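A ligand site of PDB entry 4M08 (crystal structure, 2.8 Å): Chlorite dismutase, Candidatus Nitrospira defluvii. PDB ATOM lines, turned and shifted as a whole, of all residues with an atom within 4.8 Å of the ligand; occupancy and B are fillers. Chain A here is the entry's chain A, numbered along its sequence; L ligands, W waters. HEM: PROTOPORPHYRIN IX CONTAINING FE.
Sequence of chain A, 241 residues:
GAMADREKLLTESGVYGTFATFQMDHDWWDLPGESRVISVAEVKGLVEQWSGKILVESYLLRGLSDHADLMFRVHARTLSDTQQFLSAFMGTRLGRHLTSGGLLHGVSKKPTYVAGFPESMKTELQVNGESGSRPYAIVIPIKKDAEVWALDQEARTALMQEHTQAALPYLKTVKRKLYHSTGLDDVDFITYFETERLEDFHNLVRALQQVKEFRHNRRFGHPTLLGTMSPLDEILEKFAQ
Pro 111 touches the ligand. Val 114 touches the ligand (N to O1A, 3.5 Å). Phe 117 touches the ligand. Leu 125 touches the ligand. CD1 of Ile 142 touches CAC of the ligand, 3.7 Å away. Met 160 touches the ligand (SD to CBD, 3.6 Å). Thr 164 touches the ligand. CB of Ala 167 touches C3B of the ligand (3.6 Å). Leu 171 touches the ligand (CD2 to CMB, 3.6 Å). Arg 176 touches the ligand. CD2 of Leu 178 touches C3D of the ligand, at 3.9 Å. Phe 189 touches the ligand (CZ to O1D, 3.2 Å). Thr 191 touches the ligand (CG2 to CHD, 3.7 Å). Phe 193 touches the ligand. CD2 of Leu 204 touches CBB of the ligand, 3.2 Å away. Leu 208 touches the ligand (CD1 to C2C, 3.5 Å). CE1 of Phe 220 touches CBC of the ligand, at 3.8 Å. 20 residues have an atom within 4 Å of the ligand: Pro 111, Thr 112, Tyr 113, Val 114, Phe 117, Leu 125, Ile 142, Met 160, His 163, Thr 164, Ala 167, Leu 171, Arg 176, Leu 178, Phe 189, Thr 191, Phe 193, Leu 204, Leu 208 and Phe 220. The nearest printed residue that does not touch the ligand is Trp 149 (4.1 Å).
A ring nitrogen (NE2) of His 163 is bound to an iron atom (FE) of the ligand, 2.5 Å away. The backbone NH (N) of Tyr 113 sits at hydrogen-bond distance from an oxygen (O1A) of the ligand. The backbone NH (N) of Thr 112 lies within hydrogen-bond range of an oxygen (O2A) of the ligand.
A ring nitrogen (ND1) of His 163 lies within hydrogen-bond range of the side-chain carboxylate of Glu 213 (3.3 Å). O of Phe 189 sits at hydrogen-bond distance from N of Ile 142. The guanidinium group (NH2) of Arg 176 lies within hydrogen-bond range of the backbone carbonyl oxygen (O) of Leu 125 (3.1 Å). The side-chain hydroxyl (OG1) of Thr 164 is in hydrogen-bond range of the backbone carbonyl oxygen (O) of Met 160, at 2.7 Å. N of Ile 140 lies within hydrogen-bond range of O of Thr 191, at 2.8 Å.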
ATOM      1  N   LYS A 110      21.271 -21.402  -0.520  1.00  0.00           N
ATOM      2  CA  LYS A 110      20.994 -22.819  -0.701  1.00  0.00           C
ATOM      3  C   LYS A 110      21.708 -23.615   0.371  1.00  0.00           C
ATOM      4  O   LYS A 110      22.844 -23.278   0.736  1.00  0.00           O
ATOM      5  CB  LYS A 110      21.405 -23.306  -2.094  1.00  0.00           C
ATOM      6  CG  LYS A 110      20.628 -22.671  -3.239  1.00  0.00           C
ATOM      7  CD  LYS A 110      21.246 -23.025  -4.584  1.00  0.00           C
ATOM      8  CE  LYS A 110      20.432 -22.443  -5.726  1.00  0.00           C
ATOM      9  NZ  LYS A 110      20.498 -20.948  -5.762  1.00  0.00           N
ATOM     10  N   PRO A 111      21.044 -24.638   0.917  1.00  0.00           N
ATOM     11  CA  PRO A 111      21.592 -25.474   1.989  1.00  0.00           C
ATOM     12  C   PRO A 111      22.969 -26.033   1.648  1.00  0.00           C
ATOM     13  O   PRO A 111      23.195 -26.475   0.516  1.00  0.00           O
ATOM     14  CB  PRO A 111      20.551 -26.585   2.123  1.00  0.00           C
ATOM     15  CG  PRO A 111      19.267 -25.938   1.692  1.00  0.00           C
ATOM     16  CD  PRO A 111      19.664 -25.017   0.562  1.00  0.00           C
ATOM     17  N   THR A 112      23.873 -26.025   2.619  1.00  0.00           N
ATOM     18  CA  THR A 112      25.239 -26.479   2.393  1.00  0.00           C
ATOM     19  C   THR A 112      25.489 -27.866   2.971  1.00  0.00           C
ATOM     20  O   THR A 112      26.405 -28.567   2.555  1.00  0.00           O
ATOM     21  CB  THR A 112      26.267 -25.473   2.976  1.00  0.00           C
ATOM     22  OG1 THR A 112      26.505 -25.769   4.363  1.00  0.00           O
ATOM     23  CG2 THR A 112      25.751 -24.042   2.853  1.00  0.00           C
ATOM     24  N   TYR A 113      24.655 -28.267   3.935  1.00  0.00           N
ATOM     25  CA  TYR A 113      24.837 -29.538   4.638  1.00  0.00           C
ATOM     26  C   TYR A 113      23.849 -30.619   4.182  1.00  0.00           C
ATOM     27  O   TYR A 113      24.145 -31.810   4.264  1.00  0.00           O
ATOM     28  CB  TYR A 113      24.712 -29.318   6.144  1.00  0.00           C
ATOM     29  CG  TYR A 113      25.698 -28.317   6.710  1.00  0.00           C
ATOM     30  CD1 TYR A 113      27.033 -28.343   6.342  1.00  0.00           C
ATOM     31  CD2 TYR A 113      25.282 -27.332   7.587  1.00  0.00           C
ATOM     32  CE1 TYR A 113      27.936 -27.430   6.865  1.00  0.00           C
ATOM     33  CE2 TYR A 113      26.170 -26.413   8.115  1.00  0.00           C
ATOM     34  CZ  TYR A 113      27.494 -26.473   7.743  1.00  0.00           C
ATOM     35  OH  TYR A 113      28.382 -25.554   8.254  1.00  0.00           O
ATOM     36  N   VAL A 114      22.673 -30.201   3.719  1.00  0.00           N
ATOM     37  CA  VAL A 114      21.622 -31.140   3.328  1.00  0.00           C
ATOM     38  C   VAL A 114      22.120 -32.155   2.304  1.00  0.00           C
ATOM     39  O   VAL A 114      21.682 -33.317   2.296  1.00  0.00           O
ATOM     40  CB  VAL A 114      20.402 -30.398   2.735  1.00  0.00           C
ATOM     41  CG1 VAL A 114      19.429 -31.377   2.116  1.00  0.00           C
ATOM     42  CG2 VAL A 114      19.721 -29.555   3.795  1.00  0.00           C
ATOM     43  N   PHE A 117      23.225 -35.415   3.675  1.00  0.00           N
ATOM     44  CA  PHE A 117      22.310 -36.149   4.535  1.00  0.00           C
ATOM     45  C   PHE A 117      21.861 -37.413   3.833  1.00  0.00           C
ATOM     46  O   PHE A 117      22.082 -37.568   2.637  1.00  0.00           O
ATOM     47  CB  PHE A 117      21.082 -35.300   4.908  1.00  0.00           C
ATOM     48  CG  PHE A 117      21.379 -34.114   5.785  1.00  0.00           C
ATOM     49  CD1 PHE A 117      22.648 -33.930   6.324  1.00  0.00           C
ATOM     50  CD2 PHE A 117      20.388 -33.197   6.089  1.00  0.00           C
ATOM     51  CE1 PHE A 117      22.912 -32.834   7.131  1.00  0.00           C
ATOM     52  CE2 PHE A 117      20.652 -32.108   6.908  1.00  0.00           C
ATOM     53  CZ  PHE A 117      21.907 -31.927   7.429  1.00  0.00           C
ATOM     54  N   LEU A 125      12.767 -33.233   4.091  1.00  0.00           N
ATOM     55  CA  LEU A 125      13.051 -31.819   4.278  1.00  0.00           C
ATOM     56  C   LEU A 125      12.350 -30.941   3.247  1.00  0.00           C
ATOM     57  O   LEU A 125      12.304 -29.712   3.393  1.00  0.00           O
ATOM     58  CB  LEU A 125      14.555 -31.570   4.256  1.00  0.00           C
ATOM     59  CG  LEU A 125      15.279 -31.891   5.572  1.00  0.00           C
ATOM     60  CD1 LEU A 125      16.797 -31.779   5.431  1.00  0.00           C
ATOM     61  CD2 LEU A 125      14.782 -30.981   6.689  1.00  0.00           C
ATOM     62  N   ILE A 140      14.582 -15.744  16.156  1.00  0.00           N
ATOM     63  CA  ILE A 140      15.638 -16.002  17.122  1.00  0.00           C
ATOM     64  C   ILE A 140      17.006 -15.808  16.481  1.00  0.00           C
ATOM     65  O   ILE A 140      17.470 -16.645  15.718  1.00  0.00           O
ATOM     66  CB  ILE A 140      15.516 -17.436  17.714  1.00  0.00           C
ATOM     67  CG1 ILE A 140      14.218 -17.560  18.520  1.00  0.00           C
ATOM     68  CG2 ILE A 140      16.715 -17.764  18.588  1.00  0.00           C
ATOM     69  CD1 ILE A 140      13.952 -18.969  19.050  1.00  0.00           C
ATOM     70  N   ILE A 142      21.027 -15.715  16.265  1.00  0.00           N
ATOM     71  CA  ILE A 142      21.975 -16.661  16.819  1.00  0.00           C
ATOM     72  C   ILE A 142      23.423 -16.309  16.488  1.00  0.00           C
ATOM     73  O   ILE A 142      23.776 -16.126  15.321  1.00  0.00           O
ATOM     74  CB  ILE A 142      21.646 -18.093  16.348  1.00  0.00           C
ATOM     75  CG1 ILE A 142      20.220 -18.474  16.768  1.00  0.00           C
ATOM     76  CG2 ILE A 142      22.655 -19.083  16.888  1.00  0.00           C
ATOM     77  CD1 ILE A 142      19.780 -19.867  16.351  1.00  0.00           C
ATOM     78  N   TRP A 149      33.568 -22.565  14.209  1.00  0.00           N
ATOM     79  CA  TRP A 149      34.024 -22.315  12.837  1.00  0.00           C
ATOM     80  C   TRP A 149      35.368 -22.980  12.548  1.00  0.00           C
ATOM     81  O   TRP A 149      35.837 -22.981  11.412  1.00  0.00           O
ATOM     82  CB  TRP A 149      34.100 -20.813  12.564  1.00  0.00           C
ATOM     83  CG  TRP A 149      32.821 -20.099  12.880  1.00  0.00           C
ATOM     84  CD1 TRP A 149      32.665 -18.981  13.661  1.00  0.00           C
ATOM     85  CD2 TRP A 149      31.506 -20.488  12.475  1.00  0.00           C
ATOM     86  NE1 TRP A 149      31.332 -18.636  13.727  1.00  0.00           N
ATOM     87  CE2 TRP A 149      30.609 -19.549  13.004  1.00  0.00           C
ATOM     88  CE3 TRP A 149      31.010 -21.530  11.695  1.00  0.00           C
ATOM     89  CZ2 TRP A 149      29.227 -19.624  12.787  1.00  0.00           C
ATOM     90  CZ3 TRP A 149      29.642 -21.605  11.478  1.00  0.00           C
ATOM     91  CH2 TRP A 149      28.765 -20.659  12.019  1.00  0.00           C
ATOM     92  N   MET A 160      24.642 -30.948  12.036  1.00  0.00           N
ATOM     93  CA  MET A 160      23.369 -30.483  11.482  1.00  0.00           C
ATOM     94  C   MET A 160      22.385 -31.625  11.238  1.00  0.00           C
ATOM     95  O   MET A 160      21.173 -31.431  11.279  1.00  0.00           O
ATOM     96  CB  MET A 160      23.610 -29.694  10.196  1.00  0.00           C
ATOM     97  CG  MET A 160      24.218 -28.326  10.415  1.00  0.00           C
ATOM     98  SD  MET A 160      23.233 -27.279  11.498  1.00  0.00           S
ATOM     99  CE  MET A 160      24.342 -27.103  12.895  1.00  0.00           C
ATOM    100  N   HIS A 163      21.042 -32.340  14.408  1.00  0.00           N
ATOM    101  CA  HIS A 163      20.146 -31.209  14.574  1.00  0.00           C
ATOM    102  C   HIS A 163      18.827 -31.442  13.841  1.00  0.00           C
ATOM    103  O   HIS A 163      17.751 -31.329  14.434  1.00  0.00           O
ATOM    104  CB  HIS A 163      20.828 -29.937  14.065  1.00  0.00           C
ATOM    105  CG  HIS A 163      19.930 -28.755  13.996  1.00  0.00           C
ATOM    106  ND1 HIS A 163      19.584 -28.008  15.114  1.00  0.00           N
ATOM    107  CD2 HIS A 163      19.286 -28.184  12.955  1.00  0.00           C
ATOM    108  CE1 HIS A 163      18.780 -27.033  14.746  1.00  0.00           C
ATOM    109  NE2 HIS A 163      18.584 -27.118  13.446  1.00  0.00           N
ATOM    110  N   THR A 164      18.923 -31.770  12.560  1.00  0.00           N
ATOM    111  CA  THR A 164      17.744 -32.033  11.728  1.00  0.00           C
ATOM    112  C   THR A 164      16.946 -33.214  12.240  1.00  0.00           C
ATOM    113  O   THR A 164      15.710 -33.207  12.218  1.00  0.00           O
ATOM    114  CB  THR A 164      18.135 -32.304  10.270  1.00  0.00           C
ATOM    115  OG1 THR A 164      18.981 -31.253   9.783  1.00  0.00           O
ATOM    116  CG2 THR A 164      16.884 -32.404   9.391  1.00  0.00           C
ATOM    117  N   ALA A 167      14.562 -32.456  14.888  1.00  0.00           N
ATOM    118  CA  ALA A 167      13.548 -31.503  14.466  1.00  0.00           C
ATOM    119  C   ALA A 167      12.497 -32.149  13.566  1.00  0.00           C
ATOM    120  O   ALA A 167      11.492 -31.530  13.245  1.00  0.00           O
ATOM    121  CB  ALA A 167      14.201 -30.337  13.744  1.00  0.00           C
ATOM    122  N   TYR A 170       8.575 -31.979  13.549  1.00  0.00           N
ATOM    123  CA  TYR A 170       7.949 -30.659  13.453  1.00  0.00           C
ATOM    124  C   TYR A 170       7.980 -30.044  12.052  1.00  0.00           C
ATOM    125  O   TYR A 170       7.686 -28.856  11.901  1.00  0.00           O
ATOM    126  CB  TYR A 170       8.614 -29.707  14.444  1.00  0.00           C
ATOM    127  CG  TYR A 170       8.705 -30.254  15.849  1.00  0.00           C
ATOM    128  CD1 TYR A 170       7.810 -29.854  16.827  1.00  0.00           C
ATOM    129  CD2 TYR A 170       9.682 -31.185  16.194  1.00  0.00           C
ATOM    130  CE1 TYR A 170       7.891 -30.363  18.114  1.00  0.00           C
ATOM    131  CE2 TYR A 170       9.764 -31.695  17.464  1.00  0.00           C
ATOM    132  CZ  TYR A 170       8.861 -31.285  18.424  1.00  0.00           C
ATOM    133  OH  TYR A 170       8.956 -31.786  19.699  1.00  0.00           O
ATOM    134  N   LEU A 171       8.336 -30.836  11.047  1.00  0.00           N
ATOM    135  CA  LEU A 171       8.434 -30.328   9.676  1.00  0.00           C
ATOM    136  C   LEU A 171       7.138 -29.693   9.187  1.00  0.00           C
ATOM    137  O   LEU A 171       7.154 -28.643   8.529  1.00  0.00           O
ATOM    138  CB  LEU A 171       8.842 -31.453   8.721  1.00  0.00           C
ATOM    139  CG  LEU A 171      10.298 -31.924   8.822  1.00  0.00           C
ATOM    140  CD1 LEU A 171      10.464 -33.309   8.224  1.00  0.00           C
ATOM    141  CD2 LEU A 171      11.216 -30.933   8.120  1.00  0.00           C
ATOM    142  N   VAL A 174       5.623 -26.791  12.065  1.00  0.00           N
ATOM    143  CA  VAL A 174       6.432 -25.601  12.280  1.00  0.00           C
ATOM    144  C   VAL A 174       7.160 -25.160  11.006  1.00  0.00           C
ATOM    145  O   VAL A 174       8.082 -25.850  10.555  1.00  0.00           O
ATOM    146  CB  VAL A 174       7.469 -25.827  13.400  1.00  0.00           C
ATOM    147  CG1 VAL A 174       8.432 -24.660  13.487  1.00  0.00           C
ATOM    148  CG2 VAL A 174       6.762 -26.033  14.736  1.00  0.00           C
ATOM    149  N   ARG A 176       9.780 -22.885   8.841  1.00  0.00           N
ATOM    150  CA  ARG A 176      11.133 -22.446   9.193  1.00  0.00           C
ATOM    151  C   ARG A 176      11.768 -21.635   8.068  1.00  0.00           C
ATOM    152  O   ARG A 176      11.491 -21.864   6.891  1.00  0.00           O
ATOM    153  CB  ARG A 176      12.016 -23.647   9.517  1.00  0.00           C
ATOM    154  CG  ARG A 176      12.451 -24.417   8.281  1.00  0.00           C
ATOM    155  CD  ARG A 176      13.071 -25.770   8.598  1.00  0.00           C
ATOM    156  NE  ARG A 176      13.579 -26.409   7.390  1.00  0.00           N
ATOM    157  CZ  ARG A 176      12.870 -27.228   6.616  1.00  0.00           C
ATOM    158  NH1 ARG A 176      11.622 -27.526   6.929  1.00  0.00           N
ATOM    159  NH2 ARG A 176      13.415 -27.746   5.523  1.00  0.00           N
ATOM    160  N   LEU A 178      15.800 -19.542   7.299  1.00  0.00           N
ATOM    161  CA  LEU A 178      17.127 -19.214   7.824  1.00  0.00           C
ATOM    162  C   LEU A 178      17.777 -18.089   7.034  1.00  0.00           C
ATOM    163  O   LEU A 178      17.817 -18.123   5.805  1.00  0.00           O
ATOM    164  CB  LEU A 178      18.017 -20.451   7.810  1.00  0.00           C
ATOM    165  CG  LEU A 178      19.445 -20.303   8.336  1.00  0.00           C
ATOM    166  CD1 LEU A 178      19.428 -20.016   9.828  1.00  0.00           C
ATOM    167  CD2 LEU A 178      20.248 -21.560   8.055  1.00  0.00           C
ATOM    168  N   PHE A 189      23.463 -15.817  12.457  1.00  0.00           N
ATOM    169  CA  PHE A 189      22.252 -16.290  11.786  1.00  0.00           C
ATOM    170  C   PHE A 189      21.014 -15.583  12.329  1.00  0.00           C
ATOM    171  O   PHE A 189      20.977 -15.196  13.486  1.00  0.00           O
ATOM    172  CB  PHE A 189      22.078 -17.800  11.942  1.00  0.00           C
ATOM    173  CG  PHE A 189      23.219 -18.611  11.398  1.00  0.00           C
ATOM    174  CD1 PHE A 189      23.317 -18.866  10.038  1.00  0.00           C
ATOM    175  CD2 PHE A 189      24.180 -19.127  12.250  1.00  0.00           C
ATOM    176  CE1 PHE A 189      24.360 -19.621   9.541  1.00  0.00           C
ATOM    177  CE2 PHE A 189      25.230 -19.878  11.747  1.00  0.00           C
ATOM    178  CZ  PHE A 189      25.320 -20.129  10.398  1.00  0.00           C
ATOM    179  N   THR A 191      17.089 -16.722  12.627  1.00  0.00           N
ATOM    180  CA  THR A 191      16.135 -17.804  12.425  1.00  0.00           C
ATOM    181  C   THR A 191      14.719 -17.262  12.558  1.00  0.00           C
ATOM    182  O   THR A 191      14.451 -16.410  13.405  1.00  0.00           O
ATOM    183  CB  THR A 191      16.372 -18.954  13.418  1.00  0.00           C
ATOM    184  OG1 THR A 191      16.280 -18.446  14.751  1.00  0.00           O
ATOM    185  CG2 THR A 191      17.752 -19.554  13.201  1.00  0.00           C
ATOM    186  N   PHE A 193      10.402 -18.460  12.280  1.00  0.00           N
ATOM    187  CA  PHE A 193       9.470 -19.580  12.312  1.00  0.00           C
ATOM    188  C   PHE A 193       8.021 -19.128  12.358  1.00  0.00           C
ATOM    189  O   PHE A 193       7.696 -18.091  12.938  1.00  0.00           O
ATOM    190  CB  PHE A 193       9.760 -20.486  13.511  1.00  0.00           C
ATOM    191  CG  PHE A 193      11.197 -20.835  13.679  1.00  0.00           C
ATOM    192  CD1 PHE A 193      11.759 -21.901  12.995  1.00  0.00           C
ATOM    193  CD2 PHE A 193      12.005 -20.104  14.535  1.00  0.00           C
ATOM    194  CE1 PHE A 193      13.094 -22.219  13.154  1.00  0.00           C
ATOM    195  CE2 PHE A 193      13.339 -20.414  14.699  1.00  0.00           C
ATOM    196  CZ  PHE A 193      13.880 -21.478  14.009  1.00  0.00           C
ATOM    197  N   PHE A 201       6.195 -25.555  18.966  1.00  0.00           N
ATOM    198  CA  PHE A 201       7.467 -24.857  18.791  1.00  0.00           C
ATOM    199  C   PHE A 201       8.311 -24.931  20.055  1.00  0.00           C
ATOM    200  O   PHE A 201       9.534 -25.015  19.989  1.00  0.00           O
ATOM    201  CB  PHE A 201       7.236 -23.390  18.411  1.00  0.00           C
ATOM    202  CG  PHE A 201       8.498 -22.598  18.294  1.00  0.00           C
ATOM    203  CD1 PHE A 201       9.305 -22.715  17.170  1.00  0.00           C
ATOM    204  CD2 PHE A 201       8.896 -21.747  19.309  1.00  0.00           C
ATOM    205  CE1 PHE A 201      10.474 -21.989  17.067  1.00  0.00           C
ATOM    206  CE2 PHE A 201      10.065 -21.021  19.206  1.00  0.00           C
ATOM    207  CZ  PHE A 201      10.865 -21.142  18.088  1.00  0.00           C
ATOM    208  N   LEU A 204       9.937 -28.123  20.129  1.00  0.00           N
ATOM    209  CA  LEU A 204      10.952 -28.130  19.089  1.00  0.00           C
ATOM    210  C   LEU A 204      12.278 -27.576  19.613  1.00  0.00           C
ATOM    211  O   LEU A 204      13.344 -28.158  19.372  1.00  0.00           O
ATOM    212  CB  LEU A 204      10.495 -27.335  17.871  1.00  0.00           C
ATOM    213  CG  LEU A 204      11.567 -26.962  16.839  1.00  0.00           C
ATOM    214  CD1 LEU A 204      12.131 -28.193  16.135  1.00  0.00           C
ATOM    215  CD2 LEU A 204      11.019 -25.982  15.822  1.00  0.00           C
ATOM    216  N   VAL A 205      12.207 -26.455  20.326  1.00  0.00           N
ATOM    217  CA  VAL A 205      13.405 -25.819  20.847  1.00  0.00           C
ATOM    218  C   VAL A 205      13.942 -26.622  22.015  1.00  0.00           C
ATOM    219  O   VAL A 205      15.152 -26.685  22.238  1.00  0.00           O
ATOM    220  CB  VAL A 205      13.151 -24.370  21.289  1.00  0.00           C
ATOM    221  CG1 VAL A 205      14.428 -23.739  21.812  1.00  0.00           C
ATOM    222  CG2 VAL A 205      12.585 -23.560  20.143  1.00  0.00           C
ATOM    223  N   LEU A 208      15.817 -29.547  20.581  1.00  0.00           N
ATOM    224  CA  LEU A 208      17.094 -29.144  19.990  1.00  0.00           C
ATOM    225  C   LEU A 208      18.150 -28.805  21.041  1.00  0.00           C
ATOM    226  O   LEU A 208      19.338 -28.792  20.738  1.00  0.00           O
ATOM    227  CB  LEU A 208      16.886 -27.943  19.052  1.00  0.00           C
ATOM    228  CG  LEU A 208      16.205 -28.220  17.715  1.00  0.00           C
ATOM    229  CD1 LEU A 208      16.045 -26.932  16.912  1.00  0.00           C
ATOM    230  CD2 LEU A 208      16.978 -29.249  16.911  1.00  0.00           C
ATOM    231  N   GLU A 213      25.174 -29.454  19.066  1.00  0.00           N
ATOM    232  CA  GLU A 213      25.239 -28.162  18.389  1.00  0.00           C
ATOM    233  C   GLU A 213      24.828 -27.000  19.284  1.00  0.00           C
ATOM    234  O   GLU A 213      25.359 -25.902  19.165  1.00  0.00           O
ATOM    235  CB  GLU A 213      24.341 -28.186  17.142  1.00  0.00           C
ATOM    236  CG  GLU A 213      24.123 -26.833  16.491  1.00  0.00           C
ATOM    237  CD  GLU A 213      22.669 -26.402  16.549  1.00  0.00           C
ATOM    238  OE1 GLU A 213      21.863 -27.071  17.245  1.00  0.00           O
ATOM    239  OE2 GLU A 213      22.311 -25.381  15.915  1.00  0.00           O
ATOM    240  N   PHE A 220      21.784 -16.775  22.173  1.00  0.00           N
ATOM    241  CA  PHE A 220      20.592 -17.495  21.731  1.00  0.00           C
ATOM    242  C   PHE A 220      19.367 -16.765  22.238  1.00  0.00           C
ATOM    243  O   PHE A 220      19.006 -16.858  23.412  1.00  0.00           O
ATOM    244  CB  PHE A 220      20.607 -18.934  22.239  1.00  0.00           C
ATOM    245  CG  PHE A 220      19.423 -19.736  21.797  1.00  0.00           C
ATOM    246  CD1 PHE A 220      19.387 -20.321  20.547  1.00  0.00           C
ATOM    247  CD2 PHE A 220      18.335 -19.916  22.650  1.00  0.00           C
ATOM    248  CE1 PHE A 220      18.290 -21.068  20.144  1.00  0.00           C
ATOM    249  CE2 PHE A 220      17.245 -20.657  22.258  1.00  0.00           C
ATOM    250  CZ  PHE A 220      17.215 -21.238  21.002  1.00  0.00           C
HETATM  251  CHA HEM L   1      20.616 -25.040   9.755  1.00  0.00           C
HETATM  252  CHB HEM L   1      16.904 -28.167   9.655  1.00  0.00           C
HETATM  253  CHC HEM L   1      14.736 -25.745  13.254  1.00  0.00           C
HETATM  254  CHD HEM L   1      18.769 -23.076  13.839  1.00  0.00           C
HETATM  255  C1A HEM L   1      19.787 -26.073   9.379  1.00  0.00           C
HETATM  256  C2A HEM L   1      19.971 -26.978   8.262  1.00  0.00           C
HETATM  257  C3A HEM L   1      18.950 -27.834   8.237  1.00  0.00           C
HETATM  258  C4A HEM L   1      18.068 -27.512   9.341  1.00  0.00           C
HETATM  259  CMA HEM L   1      18.751 -28.979   7.214  1.00  0.00           C
HETATM  260  CAA HEM L   1      21.142 -26.984   7.266  1.00  0.00           C
HETATM  261  CBA HEM L   1      21.158 -25.684   6.471  1.00  0.00           C
HETATM  262  CGA HEM L   1      22.202 -25.853   5.413  1.00  0.00           C
HETATM  263  O1A HEM L   1      22.654 -27.013   5.241  1.00  0.00           O
HETATM  264  O2A HEM L   1      22.585 -24.848   4.752  1.00  0.00           O
HETATM  265  C1B HEM L   1      15.941 -27.710  10.530  1.00  0.00           C
HETATM  266  C2B HEM L   1      14.552 -28.122  10.546  1.00  0.00           C
HETATM  267  C3B HEM L   1      13.945 -27.464  11.538  1.00  0.00           C
HETATM  268  C4B HEM L   1      14.930 -26.606  12.181  1.00  0.00           C
HETATM  269  CMB HEM L   1      13.906 -29.143   9.595  1.00  0.00           C
HETATM  270  CAB HEM L   1      12.442 -27.618  11.901  1.00  0.00           C
HETATM  271  CBB HEM L   1      11.878 -26.880  12.865  1.00  0.00           C
HETATM  272  C1C HEM L   1      15.670 -24.863  13.774  1.00  0.00           C
HETATM  273  C2C HEM L   1      15.524 -24.064  14.973  1.00  0.00           C
HETATM  274  C3C HEM L   1      16.632 -23.327  15.129  1.00  0.00           C
HETATM  275  C4C HEM L   1      17.526 -23.632  14.035  1.00  0.00           C
HETATM  276  CMC HEM L   1      14.290 -24.063  15.911  1.00  0.00           C
HETATM  277  CAC HEM L   1      16.949 -22.317  16.255  1.00  0.00           C
HETATM  278  CBC HEM L   1      16.061 -21.976  17.196  1.00  0.00           C
HETATM  279  C1D HEM L   1      19.643 -23.313  12.805  1.00  0.00           C
HETATM  280  C2D HEM L   1      20.912 -22.654  12.598  1.00  0.00           C
HETATM  281  C3D HEM L   1      21.490 -23.274  11.315  1.00  0.00           C
HETATM  282  C4D HEM L   1      20.507 -24.247  10.875  1.00  0.00           C
HETATM  283  CMD HEM L   1      21.566 -21.570  13.471  1.00  0.00           C
HETATM  284  CAD HEM L   1      22.844 -22.935  10.648  1.00  0.00           C
HETATM  285  CBD HEM L   1      23.881 -23.788  11.371  1.00  0.00           C
HETATM  286  CGD HEM L   1      25.255 -23.587  10.776  1.00  0.00           C
HETATM  287  O1D HEM L   1      25.359 -23.181   9.591  1.00  0.00           O
HETATM  288  O2D HEM L   1      26.251 -23.853  11.499  1.00  0.00           O
HETATM  289  NA  HEM L   1      18.605 -26.431  10.010  1.00  0.00           N
HETATM  290  NB  HEM L   1      16.134 -26.789  11.531  1.00  0.00           N
HETATM  291  NC  HEM L   1      16.907 -24.572  13.224  1.00  0.00           N
HETATM  292  ND  HEM L   1      19.436 -24.229  11.774  1.00  0.00           N
HETATM  293 FE   HEM L   1      17.792 -25.551  11.672  1.00  0.00          FE
HETATM  294  O   HOH W   1      24.080 -22.946   6.783  1.00  0.00           O
